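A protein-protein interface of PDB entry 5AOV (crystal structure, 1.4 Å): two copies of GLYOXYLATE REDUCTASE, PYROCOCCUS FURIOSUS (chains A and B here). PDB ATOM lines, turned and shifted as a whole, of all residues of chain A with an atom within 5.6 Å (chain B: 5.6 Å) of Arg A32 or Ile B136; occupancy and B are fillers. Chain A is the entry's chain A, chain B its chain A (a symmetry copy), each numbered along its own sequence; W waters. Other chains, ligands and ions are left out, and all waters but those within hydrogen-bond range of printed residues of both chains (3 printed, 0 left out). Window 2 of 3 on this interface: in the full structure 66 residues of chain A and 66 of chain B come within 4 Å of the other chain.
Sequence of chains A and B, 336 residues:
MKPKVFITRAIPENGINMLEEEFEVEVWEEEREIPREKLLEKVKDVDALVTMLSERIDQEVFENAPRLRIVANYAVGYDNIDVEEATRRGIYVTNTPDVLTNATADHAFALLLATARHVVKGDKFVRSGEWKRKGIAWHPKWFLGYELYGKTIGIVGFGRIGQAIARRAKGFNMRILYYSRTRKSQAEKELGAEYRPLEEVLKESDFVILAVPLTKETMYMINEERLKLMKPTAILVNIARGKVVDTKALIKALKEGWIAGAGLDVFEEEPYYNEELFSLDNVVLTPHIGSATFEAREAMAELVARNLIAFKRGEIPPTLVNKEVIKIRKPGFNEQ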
ATOM      1  N   ARG A   9      18.776  25.405  14.677  1.00  0.00           N
ATOM      2  CA  ARG A   9      17.919  24.637  13.800  1.00  0.00           C
ATOM      3  C   ARG A   9      17.912  25.225  12.401  1.00  0.00           C
ATOM      4  O   ARG A   9      18.234  26.393  12.211  1.00  0.00           O
ATOM      5  CB  ARG A   9      16.452  24.680  14.309  1.00  0.00           C
ATOM      6  CG  ARG A   9      15.666  23.437  14.160  1.00  0.00           C
ATOM      7  CD  ARG A   9      16.037  22.387  15.240  1.00  0.00           C
ATOM      8  NE  ARG A   9      15.213  21.166  15.204  1.00  0.00           N
ATOM      9  CZ  ARG A   9      15.541  20.054  14.575  1.00  0.00           C
ATOM     10  NH1 ARG A   9      16.666  20.019  13.836  1.00  0.00           N
ATOM     11  NH2 ARG A   9      14.793  19.008  14.702  1.00  0.00           N
ATOM     12  N   TRP A  28      22.870  24.897  13.095  1.00  0.00           N
ATOM     13  CA  TRP A  28      22.721  23.432  13.226  1.00  0.00           C
ATOM     14  C   TRP A  28      21.754  22.940  12.149  1.00  0.00           C
ATOM     15  O   TRP A  28      20.570  23.316  12.164  1.00  0.00           O
ATOM     16  CB  TRP A  28      22.164  23.177  14.636  1.00  0.00           C
ATOM     17  CG  TRP A  28      21.938  21.676  14.932  1.00  0.00           C
ATOM     18  CD1 TRP A  28      20.727  21.017  14.830  1.00  0.00           C
ATOM     19  CD2 TRP A  28      22.888  20.704  15.327  1.00  0.00           C
ATOM     20  NE1 TRP A  28      20.866  19.723  15.163  1.00  0.00           N
ATOM     21  CE2 TRP A  28      22.203  19.462  15.474  1.00  0.00           C
ATOM     22  CE3 TRP A  28      24.262  20.741  15.625  1.00  0.00           C
ATOM     23  CZ2 TRP A  28      22.831  18.336  15.916  1.00  0.00           C
ATOM     24  CZ3 TRP A  28      24.861  19.627  16.076  1.00  0.00           C
ATOM     25  CH2 TRP A  28      24.195  18.414  16.178  1.00  0.00           C
ATOM     26  N   GLU A  30      21.242  19.623  11.069  1.00  0.00           N
ATOM     27  CA  GLU A  30      20.781  18.252  11.089  1.00  0.00           C
ATOM     28  C   GLU A  30      19.278  18.108  11.340  1.00  0.00           C
ATOM     29  O   GLU A  30      18.654  18.969  11.908  1.00  0.00           O
ATOM     30  CB  GLU A  30      21.496  17.470  12.203  1.00  0.00           C
ATOM     31  CG  GLU A  30      23.000  17.369  12.031  1.00  0.00           C
ATOM     32  CD  GLU A  30      23.409  16.391  11.002  1.00  0.00           C
ATOM     33  OE1 GLU A  30      22.605  15.675  10.314  1.00  0.00           O
ATOM     34  OE2 GLU A  30      24.630  16.258  10.886  1.00  0.00           O
ATOM     35  N   GLU A  31      18.761  16.968  10.892  1.00  0.00           N
ATOM     36  CA  GLU A  31      17.333  16.658  11.133  1.00  0.00           C
ATOM     37  C   GLU A  31      17.082  16.542  12.637  1.00  0.00           C
ATOM     38  O   GLU A  31      16.110  17.101  13.120  1.00  0.00           O
ATOM     39  CB  GLU A  31      16.955  15.400  10.404  1.00  0.00           C
ATOM     40  CG  GLU A  31      15.455  15.084  10.482  1.00  0.00           C
ATOM     41  CD  GLU A  31      15.104  13.680   9.986  1.00  0.00           C
ATOM     42  OE1 GLU A  31      15.760  12.655  10.385  1.00  0.00           O
ATOM     43  OE2 GLU A  31      14.175  13.631   9.177  1.00  0.00           O
ATOM     44  N   ARG A  32      17.914  15.797  13.330  1.00  0.00           N
ATOM     45  CA  ARG A  32      17.791  15.687  14.761  1.00  0.00           C
ATOM     46  C   ARG A  32      18.089  16.951  15.499  1.00  0.00           C
ATOM     47  O   ARG A  32      18.797  17.834  15.002  1.00  0.00           O
ATOM     48  CB  ARG A  32      18.709  14.589  15.283  1.00  0.00           C
ATOM     49  CG  ARG A  32      20.181  14.971  15.148  1.00  0.00           C
ATOM     50  CD  ARG A  32      21.100  13.754  15.311  1.00  0.00           C
ATOM     51  NE  ARG A  32      22.543  14.079  15.100  1.00  0.00           N
ATOM     52  CZ  ARG A  32      23.162  14.050  13.924  1.00  0.00           C
ATOM     53  NH1 ARG A  32      22.521  13.766  12.801  1.00  0.00           N
ATOM     54  NH2 ARG A  32      24.473  14.318  13.890  1.00  0.00           N
ATOM     55  N   GLU A  33      17.504  17.098  16.695  1.00  0.00           N
ATOM     56  CA  GLU A  33      17.763  18.234  17.542  1.00  0.00           C
ATOM     57  C   GLU A  33      19.204  18.205  18.100  1.00  0.00           C
ATOM     58  O   GLU A  33      19.790  17.147  18.244  1.00  0.00           O
ATOM     59  CB  GLU A  33      16.774  18.301  18.703  1.00  0.00           C
ATOM     60  CG  GLU A  33      15.412  18.851  18.164  1.00  0.00           C
ATOM     61  CD  GLU A  33      14.183  18.184  18.523  1.00  0.00           C
ATOM     62  OE1 GLU A  33      14.115  17.080  19.119  1.00  0.00           O
ATOM     63  OE2 GLU A  33      13.128  18.840  18.199  1.00  0.00           O
ATOM     64  N   ILE A  34      19.715  19.380  18.424  1.00  0.00           N
ATOM     65  CA  ILE A  34      21.092  19.418  18.939  1.00  0.00           C
ATOM     66  C   ILE A  34      21.135  18.757  20.340  1.00  0.00           C
ATOM     67  O   ILE A  34      20.271  19.069  21.175  1.00  0.00           O
ATOM     68  CB  ILE A  34      21.592  20.888  18.987  1.00  0.00           C
ATOM     69  CG1 ILE A  34      23.089  20.812  19.343  1.00  0.00           C
ATOM     70  CG2 ILE A  34      20.797  21.797  19.953  1.00  0.00           C
ATOM     71  CD1 ILE A  34      23.726  22.193  19.130  1.00  0.00           C
ATOM     72  N   PRO A  35      22.080  17.856  20.572  1.00  0.00           N
ATOM     73  CA  PRO A  35      22.184  17.234  21.910  1.00  0.00           C
ATOM     74  C   PRO A  35      22.537  18.301  22.926  1.00  0.00           C
ATOM     75  O   PRO A  35      23.246  19.277  22.621  1.00  0.00           O
ATOM     76  CB  PRO A  35      23.308  16.236  21.741  1.00  0.00           C
ATOM     77  CG  PRO A  35      23.318  15.887  20.276  1.00  0.00           C
ATOM     78  CD  PRO A  35      22.950  17.185  19.595  1.00  0.00           C
ATOM     79  N   PRO A 271       9.005  14.402  21.681  1.00  0.00           N
ATOM     80  CA  PRO A 271       7.773  13.713  21.228  1.00  0.00           C
ATOM     81  C   PRO A 271       7.009  12.947  22.311  1.00  0.00           C
ATOM     82  O   PRO A 271       7.490  12.843  23.438  1.00  0.00           O
ATOM     83  CB  PRO A 271       8.254  12.766  20.127  1.00  0.00           C
ATOM     84  CG  PRO A 271       9.647  12.439  20.464  1.00  0.00           C
ATOM     85  CD  PRO A 271      10.213  13.693  21.037  1.00  0.00           C
ATOM     86  N   TRP B 131       6.347   9.311  15.732  1.00  0.00           N
ATOM     87  CA  TRP B 131       6.923  10.530  16.302  1.00  0.00           C
ATOM     88  C   TRP B 131       7.846  10.213  17.455  1.00  0.00           C
ATOM     89  O   TRP B 131       9.013  10.640  17.467  1.00  0.00           O
ATOM     90  CB  TRP B 131       5.778  11.433  16.723  1.00  0.00           C
ATOM     91  CG  TRP B 131       6.167  12.849  17.125  1.00  0.00           C
ATOM     92  CD1 TRP B 131       7.173  13.596  16.634  1.00  0.00           C
ATOM     93  CD2 TRP B 131       5.455  13.660  18.078  1.00  0.00           C
ATOM     94  NE1 TRP B 131       7.138  14.891  17.212  1.00  0.00           N
ATOM     95  CE2 TRP B 131       6.090  14.924  18.085  1.00  0.00           C
ATOM     96  CE3 TRP B 131       4.379  13.434  18.912  1.00  0.00           C
ATOM     97  CZ2 TRP B 131       5.643  15.976  18.904  1.00  0.00           C
ATOM     98  CZ3 TRP B 131       3.949  14.468  19.733  1.00  0.00           C
ATOM     99  CH2 TRP B 131       4.573  15.724  19.691  1.00  0.00           C
ATOM    100  N   LYS B 132       7.371   9.432  18.415  1.00  0.00           N
ATOM    101  CA  LYS B 132       8.240   9.060  19.512  1.00  0.00           C
ATOM    102  C   LYS B 132       9.456   8.252  19.059  1.00  0.00           C
ATOM    103  O   LYS B 132      10.547   8.473  19.557  1.00  0.00           O
ATOM    104  CB  LYS B 132       7.384   8.310  20.572  1.00  0.00           C
ATOM    105  CG  LYS B 132       8.100   7.873  21.861  1.00  0.00           C
ATOM    106  CD  LYS B 132       8.529   9.040  22.670  1.00  0.00           C
ATOM    107  CE  LYS B 132       9.236   8.580  23.995  1.00  0.00           C
ATOM    108  NZ  LYS B 132       9.500   9.794  24.801  1.00  0.00           N
ATOM    109  N   LYS B 134      11.125   8.153  16.334  1.00  0.00           N
ATOM    110  CA  LYS B 134      12.173   8.907  15.618  1.00  0.00           C
ATOM    111  C   LYS B 134      12.886   9.844  16.577  1.00  0.00           C
ATOM    112  O   LYS B 134      14.038  10.237  16.337  1.00  0.00           O
ATOM    113  CB  LYS B 134      11.472   9.655  14.489  1.00  0.00           C
ATOM    114  CG  LYS B 134      12.275  10.399  13.480  1.00  0.00           C
ATOM    115  CD  LYS B 134      11.289  10.811  12.240  1.00  0.00           C
ATOM    116  CE  LYS B 134      12.088  11.330  11.029  1.00  0.00           C
ATOM    117  NZ  LYS B 134      13.071  10.351  10.495  1.00  0.00           N
ATOM    118  N   GLY B 135      12.188  10.230  17.675  1.00  0.00           N
ATOM    119  CA  GLY B 135      12.918  10.926  18.736  1.00  0.00           C
ATOM    120  C   GLY B 135      13.092  12.435  18.563  1.00  0.00           C
ATOM    121  O   GLY B 135      13.789  13.036  19.339  1.00  0.00           O
ATOM    122  N   ILE B 136      12.515  12.994  17.529  1.00  0.00           N
ATOM    123  CA  ILE B 136      12.660  14.411  17.184  1.00  0.00           C
ATOM    124  C   ILE B 136      11.374  15.110  17.529  1.00  0.00           C
ATOM    125  O   ILE B 136      10.288  14.799  17.011  1.00  0.00           O
ATOM    126  CB  ILE B 136      13.003  14.569  15.698  1.00  0.00           C
ATOM    127  CG1 ILE B 136      14.276  13.855  15.411  1.00  0.00           C
ATOM    128  CG2 ILE B 136      13.110  16.062  15.325  1.00  0.00           C
ATOM    129  CD1 ILE B 136      14.659  13.791  13.935  1.00  0.00           C
ATOM    130  N   ALA B 137      11.452  16.098  18.409  1.00  0.00           N
ATOM    131  CA  ALA B 137      10.217  16.776  18.831  1.00  0.00           C
ATOM    132  C   ALA B 137       9.579  17.614  17.702  1.00  0.00           C
ATOM    133  O   ALA B 137       8.375  17.568  17.517  1.00  0.00           O
ATOM    134  CB  ALA B 137      10.493  17.691  20.027  1.00  0.00           C
ATOM    135  N   TRP B 138      10.413  18.321  16.977  1.00  0.00           N
ATOM    136  CA  TRP B 138       9.933  19.298  16.015  1.00  0.00           C
ATOM    137  C   TRP B 138      11.022  19.704  15.060  1.00  0.00           C
ATOM    138  O   TRP B 138      12.183  19.742  15.408  1.00  0.00           O
ATOM    139  CB  TRP B 138       9.522  20.518  16.854  1.00  0.00           C
ATOM    140  CG  TRP B 138       8.967  21.733  16.094  1.00  0.00           C
ATOM    141  CD1 TRP B 138       7.639  21.998  15.804  1.00  0.00           C
ATOM    142  CD2 TRP B 138       9.717  22.817  15.618  1.00  0.00           C
ATOM    143  NE1 TRP B 138       7.584  23.216  15.170  1.00  0.00           N
ATOM    144  CE2 TRP B 138       8.813  23.738  14.991  1.00  0.00           C
ATOM    145  CE3 TRP B 138      11.081  23.132  15.615  1.00  0.00           C
ATOM    146  CZ2 TRP B 138       9.276  24.958  14.503  1.00  0.00           C
ATOM    147  CZ3 TRP B 138      11.515  24.322  15.115  1.00  0.00           C
ATOM    148  CH2 TRP B 138      10.613  25.223  14.591  1.00  0.00           C
ATOM    149  N   HIS B 139      10.618  20.054  13.836  1.00  0.00           N
ATOM    150  CA  HIS B 139      11.543  20.532  12.829  1.00  0.00           C
ATOM    151  C   HIS B 139      10.851  21.670  12.070  1.00  0.00           C
ATOM    152  O   HIS B 139       9.673  21.570  11.733  1.00  0.00           O
ATOM    153  CB  HIS B 139      11.952  19.445  11.858  1.00  0.00           C
ATOM    154  CG  HIS B 139      13.075  19.811  10.970  1.00  0.00           C
ATOM    155  ND1 HIS B 139      12.925  20.661   9.883  1.00  0.00           N
ATOM    156  CD2 HIS B 139      14.358  19.422  10.992  1.00  0.00           C
ATOM    157  CE1 HIS B 139      14.114  20.791   9.306  1.00  0.00           C
ATOM    158  NE2 HIS B 139      15.008  20.036   9.946  1.00  0.00           N
ATOM    159  N   TRP B 142       8.818  20.576   8.878  1.00  0.00           N
ATOM    160  CA  TRP B 142       7.863  19.487   8.912  1.00  0.00           C
ATOM    161  C   TRP B 142       6.419  19.971   8.857  1.00  0.00           C
ATOM    162  O   TRP B 142       5.999  20.947   9.535  1.00  0.00           O
ATOM    163  CB  TRP B 142       7.987  18.670  10.228  1.00  0.00           C
ATOM    164  CG  TRP B 142       9.185  17.790  10.300  1.00  0.00           C
ATOM    165  CD1 TRP B 142      10.196  17.650   9.380  1.00  0.00           C
ATOM    166  CD2 TRP B 142       9.458  16.847  11.348  1.00  0.00           C
ATOM    167  NE1 TRP B 142      11.130  16.702   9.826  1.00  0.00           N
ATOM    168  CE2 TRP B 142      10.672  16.213  11.023  1.00  0.00           C
ATOM    169  CE3 TRP B 142       8.797  16.527  12.539  1.00  0.00           C
ATOM    170  CZ2 TRP B 142      11.219  15.192  11.818  1.00  0.00           C
ATOM    171  CZ3 TRP B 142       9.382  15.543  13.349  1.00  0.00           C
ATOM    172  CH2 TRP B 142      10.551  14.928  12.987  1.00  0.00           C
HETATM  173  O   HOH W   1      13.405  21.516  17.507  1.00  0.00           O
HETATM  174  O   HOH W   2      16.367  14.745  18.210  1.00  0.00           O
HETATM  175  O   HOH W   3      10.060  12.443  24.561  1.00  0.00           O
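The guanidinium group of Arg A9 is in hydrogen-bond range of the backbone carbonyl oxygen of Trp B138 (2.8 Å).
OE1 of Glu A31 is in salt-bridge range of NZ of Lys B134, 3.5 Å away.
The backbone NH (N) of Ala B137 lies within hydrogen-bond range of the side-chain carboxylate (OE1) of Glu A33.
OE2 of Glu A33 sits at hydrogen-bond distance from N of Trp B138 (3.0 Å).
The indole nitrogen of Trp B131 is in hydrogen-bond range of the backbone carbonyl oxygen of Ile B136 (3.2 Å).
NH2 of Arg A9 is in salt-bridge range of OE2 of Glu A33, at 3.9 Å.
The indole nitrogen (NE1) of Trp B131 sits at hydrogen-bond distance from the backbone carbonyl oxygen (O) of Ala B137 (3.0 Å).
The indole nitrogen of Trp A28 is in hydrogen-bond range of the backbone carbonyl oxygen of Arg A32 (2.8 Å).
NH1 of Arg A32 lies within salt-bridge range of OE1 of Glu A30 (3.1 Å).
The backbone carbonyl oxygen (O) of Arg A32 is in hydrogen-bond range of the guanidinium group (NH1) of Arg A9 (3.3 Å).
Arg A9 touches Ile B136.
Arg A9 touches His B139 (NH1 to CD2, 3.7 Å).
Glu A31 touches Ile B136 (O to CD1, 3.7 Å).
CD2 of His B139 touches O of Glu A31, at 3.6 Å.
Ile B136 touches Glu A33.
CB of Pro A271 touches O of Trp B131, at 3.5 Å.
Lys B132 touches Pro A271 (CA to CB, 3.8 Å).
Pro A271 touches Gly B135 (CG to C, 3.9 Å).
Pro A271 touches Ile B136 (CD to C, 3.96 Å).
Pro A271 touches Ala B137.
Ile B136 touches just these residues of chain A: Arg A9 (3.4 Å), Glu A31 (3.7 Å), Arg A32 (3.8 Å), Glu A33 (3.6 Å) and Pro A271 (3.96 Å).
Printed residues of chain A within 4 Å of Gly B135: Pro A271.
Printed residues of chain A within 4 Å of Lys B132: Pro A271.
Printed residues of chain B within 4 Å of Glu A31: Lys B134, Ile B136 and His B139.
Of the printed residues of chain A, Trp B138 touches Arg A9 and Glu A33.
Of the printed residues of chain B, Pro A271 touches Trp B131, Lys B132, Gly B135, Ile B136 and Ala B137.
Glu A30 touches none of the printed residues of chain B.
Pro A35 touches none of the printed residues of chain B.
The nearest printed residue of chain A that does not touch Gly B135 is Glu A33 (4.1 Å).
Of the 9 printed residues of chain A, 5 touch a printed residue of chain B.
Hydrophobic or aromatic side chains of chain A that line the printed part of chain B: Pro A271.
Among the printed residues, Asp or Glu carboxylates within 4 Å of a Lys or Arg side-chain nitrogen of the other chain: Glu A31 with Lys B134 (3.5 Å).
No position is printed for both chains.
Of the 15 pairs that touch across the chains among the printed residues, none has its exchanged pair printed and touching as well.
Water W3 bridges the side-chain amino group (NZ) of Lys B132 (2.7 Å) and the backbone carbonyl oxygen (O) of Pro A271 (2.8 Å).
Water W1 lies within hydrogen-bond range of OE2 of Glu A33 (2.8 Å), NE of Arg A9 (2.9 Å) and O of Trp B138 (3.0 Å).
Water W2 lies within hydrogen-bond range of the backbone NH (N) of Glu A33 (3.0 Å) and the backbone carbonyl oxygen (O) of Gly B135 (3.3 Å).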
